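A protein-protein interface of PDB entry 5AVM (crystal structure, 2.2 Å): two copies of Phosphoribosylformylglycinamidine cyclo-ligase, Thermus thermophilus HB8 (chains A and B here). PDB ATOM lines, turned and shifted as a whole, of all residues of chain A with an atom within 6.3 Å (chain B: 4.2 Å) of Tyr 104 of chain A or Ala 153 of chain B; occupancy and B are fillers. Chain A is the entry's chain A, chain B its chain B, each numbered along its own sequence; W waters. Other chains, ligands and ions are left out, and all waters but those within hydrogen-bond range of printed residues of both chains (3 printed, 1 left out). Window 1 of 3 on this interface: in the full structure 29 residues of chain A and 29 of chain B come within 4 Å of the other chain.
Leu 102 of chain A touches Thr 60 of chain B (CD2 to N, 3.8 Å).
Thr 60 of chain B touches Asp 103 of chain A.
Ala 153 of chain B touches Tyr 104 of chain A (CB to CE2, 3.5 Å).
CB of Ala 106 of chain A touches OD2 of Asp 151 of chain B, at 3.6 Å.
C of Gly 136 of chain A touches CG2 of Thr 60 of chain B, 3.8 Å away.
CB of Glu 137 of chain A touches O of Thr 60 of chain B, at 3.1 Å.
CE of Met 141 of chain A touches OD2 of Asp 151 of chain B (3.4 Å).
OD2 of Asp 151 of chain A touches CE2 of Tyr 104 of chain B, 3.9 Å away.
Tyr 104 of chain B touches Ala 153 of chain A.
Of the printed residues of chain B, Leu 102 of chain A touches Thr 60.
Of the printed residues of chain B, Asp 103 of chain A touches Thr 60 (3.2 Å).
Of chain B, only Asp 151 (3.0 Å) and Ala 153 (3.5 Å) come within 4 Å of Tyr 104 of chain A.
Ala 139 of chain A touches none of the printed residues of chain B.
Of the printed residues of chain B, Tyr 145 of chain A touches Asp 151.
Of chain A, only Tyr 104 (3.5 Å) comes within 4 Å of Ala 153 of chain B.
The nearest residue of chain A that does not touch Ala 153 of chain B is Ala 153 of chain A (6.1 Å).
Water W3 lies within hydrogen-bond range of OD2 of Asp 151 of chain A (2.5 Å), OH of Tyr 145 of chain A (3.4 Å) and OD2 of Asp 151 of chain B (3.5 Å).
Water W2 bridges the backbone carbonyl oxygen (O) of Gly 136 of chain A and the backbone NH (N) of Thr 60 of chain B.
Water W1 bridges OE2 of Glu 137 of chain A (3.1 Å) and OD1 of Asp 61 of chain B (3.3 Å).
Of the 10 printed residues of chain B, 5 touch a printed residue of chain A.
Printed residues of chain B that touch a printed residue of chain A: Thr 60, Asp 61, Tyr 104, Asp 151 and Ala 153.
Hydrophobic or aromatic side chains of chain B that line the printed part of chain A: Tyr 104 and Ala 153.
Of the 19 printed residues of chain A, 10 touch a printed residue of chain B.
Along chain A the printed residues that touch a printed residue of chain B span positions 102 to 153.
Among the printed residues, no Asp or Glu carboxylate lies within 4 Å of a Lys or Arg side-chain nitrogen of the other chain.
The backbone carbonyl oxygen (O) of Asp 103 of chain A lies within hydrogen-bond range of the backbone NH (N) of Glu 137 of chain A, 2.8 Å away.
The backbone NH (N) of Tyr 104 of chain A sits at hydrogen-bond distance from the backbone carbonyl oxygen (O) of Ala 153 of chain A, at 2.7 Å.
O of Ala 106 of chain A sits at hydrogen-bond distance from N of Asp 151 of chain A (3.2 Å).
The side-chain hydroxyl (OG1) of Thr 60 of chain B sits at hydrogen-bond distance from the backbone carbonyl oxygen (O) of Gly 154 of chain B (2.7 Å).
The backbone carbonyl oxygen (O) of Asp 61 of chain B is in hydrogen-bond range of the backbone NH (N) of Gly 154 of chain B (2.9 Å).
The backbone carbonyl oxygen (O) of Ala 153 of chain B is in hydrogen-bond range of the backbone NH (N) of Tyr 104 of chain B.
Tyr 104 of chain A touches Asp 151 of chain B, and with the chains exchanged Asp 151 of chain A touches Tyr 104 of chain B.
Tyr 104 of chain A touches Ala 153 of chain B, and with the chains exchanged Ala 153 of chain A touches Tyr 104 of chain B.
7 positions are printed for both chains.
OH of Tyr 104 of chain A sits at hydrogen-bond distance from OD1 of Asp 151 of chain B, 3.0 Å away.
OD2 of Asp 151 of chain B lies within hydrogen-bond range of OH of Tyr 145 of chain A (2.7 Å).
OE2 of Glu 137 of chain A sits close to OD1 of Asp 61 of chain B, 3.1 Å away.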
ATOM      1  N   LEU A  83     -13.552  -5.739  -2.167  1.00  0.00           N
ATOM      2  CA  LEU A  83     -12.700  -6.475  -1.239  1.00  0.00           C
ATOM      3  C   LEU A  83     -11.228  -6.522  -1.660  1.00  0.00           C
ATOM      4  O   LEU A  83     -10.359  -6.038  -0.938  1.00  0.00           O
ATOM      5  CB  LEU A  83     -13.228  -7.902  -1.055  1.00  0.00           C
ATOM      6  CG  LEU A  83     -12.437  -8.800  -0.095  1.00  0.00           C
ATOM      7  CD1 LEU A  83     -12.324  -8.109   1.255  1.00  0.00           C
ATOM      8  CD2 LEU A  83     -13.121 -10.163   0.055  1.00  0.00           C
ATOM      9  N   PHE A 101      -4.417 -13.976  -3.297  1.00  0.00           N
ATOM     10  CA  PHE A 101      -5.585 -13.666  -2.474  1.00  0.00           C
ATOM     11  C   PHE A 101      -6.414 -14.891  -2.081  1.00  0.00           C
ATOM     12  O   PHE A 101      -6.460 -15.894  -2.800  1.00  0.00           O
ATOM     13  CB  PHE A 101      -6.484 -12.673  -3.224  1.00  0.00           C
ATOM     14  CG  PHE A 101      -7.482 -11.967  -2.352  1.00  0.00           C
ATOM     15  CD1 PHE A 101      -7.140 -10.790  -1.693  1.00  0.00           C
ATOM     16  CD2 PHE A 101      -8.766 -12.472  -2.187  1.00  0.00           C
ATOM     17  CE1 PHE A 101      -8.061 -10.126  -0.886  1.00  0.00           C
ATOM     18  CE2 PHE A 101      -9.700 -11.813  -1.379  1.00  0.00           C
ATOM     19  CZ  PHE A 101      -9.343 -10.637  -0.728  1.00  0.00           C
ATOM     20  N   LEU A 102      -7.056 -14.797  -0.918  1.00  0.00           N
ATOM     21  CA  LEU A 102      -7.914 -15.855  -0.391  1.00  0.00           C
ATOM     22  C   LEU A 102      -9.145 -15.172   0.162  1.00  0.00           C
ATOM     23  O   LEU A 102      -9.039 -14.143   0.826  1.00  0.00           O
ATOM     24  CB  LEU A 102      -7.230 -16.634   0.738  1.00  0.00           C
ATOM     25  CG  LEU A 102      -6.166 -17.656   0.349  1.00  0.00           C
ATOM     26  CD1 LEU A 102      -4.791 -17.049   0.443  1.00  0.00           C
ATOM     27  CD2 LEU A 102      -6.262 -18.831   1.280  1.00  0.00           C
ATOM     28  N   ASP A 103     -10.312 -15.741  -0.104  1.00  0.00           N
ATOM     29  CA  ASP A 103     -11.544 -15.143   0.380  1.00  0.00           C
ATOM     30  C   ASP A 103     -12.276 -16.008   1.391  1.00  0.00           C
ATOM     31  O   ASP A 103     -12.184 -17.239   1.386  1.00  0.00           O
ATOM     32  CB  ASP A 103     -12.485 -14.850  -0.786  1.00  0.00           C
ATOM     33  CG  ASP A 103     -12.987 -16.110  -1.448  1.00  0.00           C
ATOM     34  OD1 ASP A 103     -12.174 -16.800  -2.099  1.00  0.00           O
ATOM     35  OD2 ASP A 103     -14.192 -16.416  -1.309  1.00  0.00           O
ATOM     36  N   TYR A 104     -13.008 -15.329   2.262  1.00  0.00           N
ATOM     37  CA  TYR A 104     -13.812 -15.971   3.283  1.00  0.00           C
ATOM     38  C   TYR A 104     -15.181 -15.286   3.240  1.00  0.00           C
ATOM     39  O   TYR A 104     -15.283 -14.076   3.449  1.00  0.00           O
ATOM     40  CB  TYR A 104     -13.169 -15.791   4.663  1.00  0.00           C
ATOM     41  CG  TYR A 104     -14.034 -16.281   5.803  1.00  0.00           C
ATOM     42  CD1 TYR A 104     -14.297 -17.644   5.976  1.00  0.00           C
ATOM     43  CD2 TYR A 104     -14.626 -15.377   6.686  1.00  0.00           C
ATOM     44  CE1 TYR A 104     -15.131 -18.087   7.002  1.00  0.00           C
ATOM     45  CE2 TYR A 104     -15.459 -15.811   7.711  1.00  0.00           C
ATOM     46  CZ  TYR A 104     -15.709 -17.165   7.864  1.00  0.00           C
ATOM     47  OH  TYR A 104     -16.541 -17.588   8.881  1.00  0.00           O
ATOM     48  N   LEU A 105     -16.223 -16.061   2.944  1.00  0.00           N
ATOM     49  CA  LEU A 105     -17.583 -15.535   2.873  1.00  0.00           C
ATOM     50  C   LEU A 105     -18.459 -16.299   3.863  1.00  0.00           C
ATOM     51  O   LEU A 105     -18.424 -17.531   3.909  1.00  0.00           O
ATOM     52  CB  LEU A 105     -18.142 -15.715   1.459  1.00  0.00           C
ATOM     53  CG  LEU A 105     -17.226 -15.307   0.306  1.00  0.00           C
ATOM     54  CD1 LEU A 105     -17.824 -15.779  -1.014  1.00  0.00           C
ATOM     55  CD2 LEU A 105     -17.028 -13.801   0.323  1.00  0.00           C
ATOM     56  N   ALA A 106     -19.240 -15.570   4.654  1.00  0.00           N
ATOM     57  CA  ALA A 106     -20.128 -16.189   5.629  1.00  0.00           C
ATOM     58  C   ALA A 106     -21.524 -15.577   5.511  1.00  0.00           C
ATOM     59  O   ALA A 106     -21.674 -14.448   5.054  1.00  0.00           O
ATOM     60  CB  ALA A 106     -19.580 -16.002   7.029  1.00  0.00           C
ATOM     61  N   LEU A 122     -14.998 -11.797  -7.200  1.00  0.00           N
ATOM     62  CA  LEU A 122     -13.666 -11.931  -6.606  1.00  0.00           C
ATOM     63  C   LEU A 122     -12.619 -12.391  -7.616  1.00  0.00           C
ATOM     64  O   LEU A 122     -11.499 -11.897  -7.629  1.00  0.00           O
ATOM     65  CB  LEU A 122     -13.705 -12.934  -5.456  1.00  0.00           C
ATOM     66  CG  LEU A 122     -14.467 -12.529  -4.203  1.00  0.00           C
ATOM     67  CD1 LEU A 122     -14.899 -13.784  -3.462  1.00  0.00           C
ATOM     68  CD2 LEU A 122     -13.592 -11.633  -3.329  1.00  0.00           C
ATOM     69  N   GLY A 136     -10.006 -20.354  -0.578  1.00  0.00           N
ATOM     70  CA  GLY A 136     -11.214 -19.678  -0.145  1.00  0.00           C
ATOM     71  C   GLY A 136     -11.973 -20.549   0.829  1.00  0.00           C
ATOM     72  O   GLY A 136     -11.696 -21.739   0.951  1.00  0.00           O
ATOM     73  N   GLU A 137     -12.916 -19.961   1.544  1.00  0.00           N
ATOM     74  CA  GLU A 137     -13.701 -20.725   2.489  1.00  0.00           C
ATOM     75  C   GLU A 137     -15.077 -20.116   2.496  1.00  0.00           C
ATOM     76  O   GLU A 137     -15.244 -18.946   2.155  1.00  0.00           O
ATOM     77  CB  GLU A 137     -13.086 -20.661   3.887  1.00  0.00           C
ATOM     78  CG  GLU A 137     -13.764 -21.556   4.919  1.00  0.00           C
ATOM     79  CD  GLU A 137     -13.849 -23.013   4.476  1.00  0.00           C
ATOM     80  OE1 GLU A 137     -14.691 -23.337   3.607  1.00  0.00           O
ATOM     81  OE2 GLU A 137     -13.070 -23.838   4.993  1.00  0.00           O
ATOM     82  N   THR A 138     -16.068 -20.915   2.863  1.00  0.00           N
ATOM     83  CA  THR A 138     -17.434 -20.439   2.899  1.00  0.00           C
ATOM     84  C   THR A 138     -18.099 -20.929   4.159  1.00  0.00           C
ATOM     85  O   THR A 138     -17.871 -22.057   4.585  1.00  0.00           O
ATOM     86  CB  THR A 138     -18.217 -20.938   1.688  1.00  0.00           C
ATOM     87  OG1 THR A 138     -17.615 -20.429   0.494  1.00  0.00           O
ATOM     88  CG2 THR A 138     -19.634 -20.456   1.753  1.00  0.00           C
ATOM     89  N   ALA A 139     -18.914 -20.070   4.755  1.00  0.00           N
ATOM     90  CA  ALA A 139     -19.605 -20.413   5.984  1.00  0.00           C
ATOM     91  C   ALA A 139     -21.083 -20.056   5.956  1.00  0.00           C
ATOM     92  O   ALA A 139     -21.484 -19.021   5.420  1.00  0.00           O
ATOM     93  CB  ALA A 139     -18.930 -19.729   7.173  1.00  0.00           C
ATOM     94  N   MET A 141     -23.964 -19.776   8.756  1.00  0.00           N
ATOM     95  CA  MET A 141     -24.261 -19.787  10.181  1.00  0.00           C
ATOM     96  C   MET A 141     -25.447 -18.902  10.556  1.00  0.00           C
ATOM     97  O   MET A 141     -25.266 -17.809  11.095  1.00  0.00           O
ATOM     98  CB  MET A 141     -23.020 -19.341  10.961  1.00  0.00           C
ATOM     99  CG  MET A 141     -21.749 -20.106  10.594  1.00  0.00           C
ATOM    100  SD  MET A 141     -20.388 -19.759  11.713  1.00  0.00           S
ATOM    101  CE  MET A 141     -19.605 -18.401  10.882  1.00  0.00           C
ATOM    102  N   TYR A 145     -25.372 -14.932  11.851  1.00  0.00           N
ATOM    103  CA  TYR A 145     -25.794 -13.825  11.006  1.00  0.00           C
ATOM    104  C   TYR A 145     -27.287 -13.549  11.036  1.00  0.00           C
ATOM    105  O   TYR A 145     -28.103 -14.465  11.163  1.00  0.00           O
ATOM    106  CB  TYR A 145     -25.341 -14.086   9.563  1.00  0.00           C
ATOM    107  CG  TYR A 145     -23.851 -13.901   9.387  1.00  0.00           C
ATOM    108  CD1 TYR A 145     -23.309 -12.628   9.210  1.00  0.00           C
ATOM    109  CD2 TYR A 145     -22.973 -14.982   9.485  1.00  0.00           C
ATOM    110  CE1 TYR A 145     -21.937 -12.431   9.143  1.00  0.00           C
ATOM    111  CE2 TYR A 145     -21.594 -14.793   9.421  1.00  0.00           C
ATOM    112  CZ  TYR A 145     -21.084 -13.510   9.253  1.00  0.00           C
ATOM    113  OH  TYR A 145     -19.722 -13.298   9.209  1.00  0.00           O
ATOM    114  N   ASP A 151     -21.058 -11.354   5.017  1.00  0.00           N
ATOM    115  CA  ASP A 151     -19.823 -10.656   5.340  1.00  0.00           C
ATOM    116  C   ASP A 151     -18.776 -11.149   4.365  1.00  0.00           C
ATOM    117  O   ASP A 151     -18.514 -12.342   4.275  1.00  0.00           O
ATOM    118  CB  ASP A 151     -19.359 -10.912   6.775  1.00  0.00           C
ATOM    119  CG  ASP A 151     -18.118 -10.094   7.137  1.00  0.00           C
ATOM    120  OD1 ASP A 151     -18.066  -8.889   6.796  1.00  0.00           O
ATOM    121  OD2 ASP A 151     -17.190 -10.647   7.765  1.00  0.00           O
ATOM    122  N   ILE A 152     -18.204 -10.214   3.618  1.00  0.00           N
ATOM    123  CA  ILE A 152     -17.187 -10.515   2.625  1.00  0.00           C
ATOM    124  C   ILE A 152     -15.825 -10.192   3.217  1.00  0.00           C
ATOM    125  O   ILE A 152     -15.498  -9.026   3.431  1.00  0.00           O
ATOM    126  CB  ILE A 152     -17.367  -9.646   1.358  1.00  0.00           C
ATOM    127  CG1 ILE A 152     -18.846  -9.555   0.966  1.00  0.00           C
ATOM    128  CG2 ILE A 152     -16.550 -10.224   0.219  1.00  0.00           C
ATOM    129  CD1 ILE A 152     -19.448 -10.850   0.480  1.00  0.00           C
ATOM    130  N   ALA A 153     -15.030 -11.218   3.491  1.00  0.00           N
ATOM    131  CA  ALA A 153     -13.700 -11.005   4.048  1.00  0.00           C
ATOM    132  C   ALA A 153     -12.666 -11.751   3.206  1.00  0.00           C
ATOM    133  O   ALA A 153     -13.018 -12.619   2.402  1.00  0.00           O
ATOM    134  CB  ALA A 153     -13.649 -11.475   5.507  1.00  0.00           C
ATOM    135  N   GLY A 154     -11.397 -11.402   3.382  1.00  0.00           N
ATOM    136  CA  GLY A 154     -10.347 -12.048   2.625  1.00  0.00           C
ATOM    137  C   GLY A 154      -8.974 -11.649   3.114  1.00  0.00           C
ATOM    138  O   GLY A 154      -8.840 -10.761   3.956  1.00  0.00           O
ATOM    139  N   THR A 155      -7.954 -12.308   2.570  1.00  0.00           N
ATOM    140  CA  THR A 155      -6.567 -12.057   2.938  1.00  0.00           C
ATOM    141  C   THR A 155      -5.711 -11.935   1.686  1.00  0.00           C
ATOM    142  O   THR A 155      -5.766 -12.787   0.804  1.00  0.00           O
ATOM    143  CB  THR A 155      -6.003 -13.217   3.802  1.00  0.00           C
ATOM    144  OG1 THR A 155      -6.765 -13.324   5.005  1.00  0.00           O
ATOM    145  CG2 THR A 155      -4.539 -12.980   4.165  1.00  0.00           C
ATOM    146  N   THR B  60      -7.818 -20.449   4.383  1.00  0.00           N
ATOM    147  CA  THR B  60      -8.517 -19.495   5.226  1.00  0.00           C
ATOM    148  C   THR B  60      -9.676 -20.286   5.846  1.00  0.00           C
ATOM    149  O   THR B  60     -10.318 -21.089   5.165  1.00  0.00           O
ATOM    150  CB  THR B  60      -9.019 -18.270   4.420  1.00  0.00           C
ATOM    151  OG1 THR B  60      -9.385 -17.235   5.341  1.00  0.00           O
ATOM    152  CG2 THR B  60     -10.212 -18.628   3.532  1.00  0.00           C
ATOM    153  N   ASP B  61      -9.923 -20.090   7.139  1.00  0.00           N
ATOM    154  CA  ASP B  61     -10.974 -20.838   7.842  1.00  0.00           C
ATOM    155  C   ASP B  61     -11.686 -19.985   8.863  1.00  0.00           C
ATOM    156  O   ASP B  61     -11.295 -18.854   9.119  1.00  0.00           O
ATOM    157  CB  ASP B  61     -10.375 -22.036   8.600  1.00  0.00           C
ATOM    158  CG  ASP B  61      -9.895 -23.137   7.687  1.00  0.00           C
ATOM    159  OD1 ASP B  61     -10.740 -23.787   7.043  1.00  0.00           O
ATOM    160  OD2 ASP B  61      -8.672 -23.364   7.613  1.00  0.00           O
ATOM    161  N   GLY B  62     -12.721 -20.562   9.459  1.00  0.00           N
ATOM    162  CA  GLY B  62     -13.481 -19.880  10.487  1.00  0.00           C
ATOM    163  C   GLY B  62     -13.708 -20.863  11.617  1.00  0.00           C
ATOM    164  O   GLY B  62     -13.719 -22.070  11.386  1.00  0.00           O
ATOM    165  N   LEU B  83      -9.218 -22.326  15.876  1.00  0.00           N
ATOM    166  CA  LEU B  83      -8.956 -21.716  14.571  1.00  0.00           C
ATOM    167  C   LEU B  83      -7.570 -22.041  14.008  1.00  0.00           C
ATOM    168  O   LEU B  83      -7.435 -22.504  12.875  1.00  0.00           O
ATOM    169  CB  LEU B  83      -9.115 -20.196  14.665  1.00  0.00           C
ATOM    170  CG  LEU B  83      -8.849 -19.427  13.372  1.00  0.00           C
ATOM    171  CD1 LEU B  83      -9.670 -20.019  12.232  1.00  0.00           C
ATOM    172  CD2 LEU B  83      -9.189 -17.969  13.591  1.00  0.00           C
ATOM    173  N   ASP B 103      -5.595 -12.920  11.507  1.00  0.00           N
ATOM    174  CA  ASP B 103      -7.039 -13.117  11.625  1.00  0.00           C
ATOM    175  C   ASP B 103      -7.979 -11.927  11.446  1.00  0.00           C
ATOM    176  O   ASP B 103      -7.570 -10.772  11.536  1.00  0.00           O
ATOM    177  CB  ASP B 103      -7.323 -13.744  12.985  1.00  0.00           C
ATOM    178  CG  ASP B 103      -6.639 -12.998  14.119  1.00  0.00           C
ATOM    179  OD1 ASP B 103      -6.828 -11.764  14.223  1.00  0.00           O
ATOM    180  OD2 ASP B 103      -5.910 -13.639  14.909  1.00  0.00           O
ATOM    181  N   TYR B 104      -9.257 -12.242  11.223  1.00  0.00           N
ATOM    182  CA  TYR B 104     -10.306 -11.242  11.041  1.00  0.00           C
ATOM    183  C   TYR B 104     -11.487 -11.513  11.968  1.00  0.00           C
ATOM    184  O   TYR B 104     -12.354 -12.325  11.639  1.00  0.00           O
ATOM    185  CB  TYR B 104     -10.827 -11.270   9.612  1.00  0.00           C
ATOM    186  CG  TYR B 104     -11.636 -10.050   9.248  1.00  0.00           C
ATOM    187  CD1 TYR B 104     -11.009  -8.824   9.028  1.00  0.00           C
ATOM    188  CD2 TYR B 104     -13.024 -10.116   9.115  1.00  0.00           C
ATOM    189  CE1 TYR B 104     -11.732  -7.690   8.679  1.00  0.00           C
ATOM    190  CE2 TYR B 104     -13.769  -8.984   8.766  1.00  0.00           C
ATOM    191  CZ  TYR B 104     -13.111  -7.771   8.549  1.00  0.00           C
ATOM    192  OH  TYR B 104     -13.817  -6.637   8.196  1.00  0.00           O
ATOM    193  N   ASP B 151     -17.720 -13.886  14.872  1.00  0.00           N
ATOM    194  CA  ASP B 151     -17.273 -14.753  13.793  1.00  0.00           C
ATOM    195  C   ASP B 151     -15.755 -14.677  13.851  1.00  0.00           C
ATOM    196  O   ASP B 151     -15.162 -13.611  13.683  1.00  0.00           O
ATOM    197  CB  ASP B 151     -17.767 -14.261  12.434  1.00  0.00           C
ATOM    198  CG  ASP B 151     -17.520 -15.268  11.325  1.00  0.00           C
ATOM    199  OD1 ASP B 151     -16.540 -16.027  11.415  1.00  0.00           O
ATOM    200  OD2 ASP B 151     -18.296 -15.298  10.351  1.00  0.00           O
ATOM    201  N   ILE B 152     -15.130 -15.815  14.108  1.00  0.00           N
ATOM    202  CA  ILE B 152     -13.689 -15.886  14.218  1.00  0.00           C
ATOM    203  C   ILE B 152     -13.140 -16.613  12.998  1.00  0.00           C
ATOM    204  O   ILE B 152     -13.342 -17.818  12.833  1.00  0.00           O
ATOM    205  CB  ILE B 152     -13.313 -16.627  15.515  1.00  0.00           C
ATOM    206  CG1 ILE B 152     -14.011 -15.941  16.696  1.00  0.00           C
ATOM    207  CG2 ILE B 152     -11.801 -16.660  15.695  1.00  0.00           C
ATOM    208  CD1 ILE B 152     -13.906 -16.682  18.001  1.00  0.00           C
ATOM    209  N   ALA B 153     -12.466 -15.856  12.134  1.00  0.00           N
ATOM    210  CA  ALA B 153     -11.879 -16.393  10.914  1.00  0.00           C
ATOM    211  C   ALA B 153     -10.409 -16.029  10.873  1.00  0.00           C
ATOM    212  O   ALA B 153      -9.949 -15.206  11.656  1.00  0.00           O
ATOM    213  CB  ALA B 153     -12.585 -15.830   9.705  1.00  0.00           C
ATOM    214  N   GLY B 154      -9.668 -16.653   9.963  1.00  0.00           N
ATOM    215  CA  GLY B 154      -8.252 -16.369   9.857  1.00  0.00           C
ATOM    216  C   GLY B 154      -7.642 -16.957   8.605  1.00  0.00           C
ATOM    217  O   GLY B 154      -8.342 -17.529   7.766  1.00  0.00           O
HETATM  218  O   HOH W   1     -12.531 -26.484   6.591  1.00  0.00           O
HETATM  219  O   HOH W   2      -8.890 -21.915   1.858  1.00  0.00           O
HETATM  220  O   HOH W   3     -16.426 -12.767   8.877  1.00  0.00           O
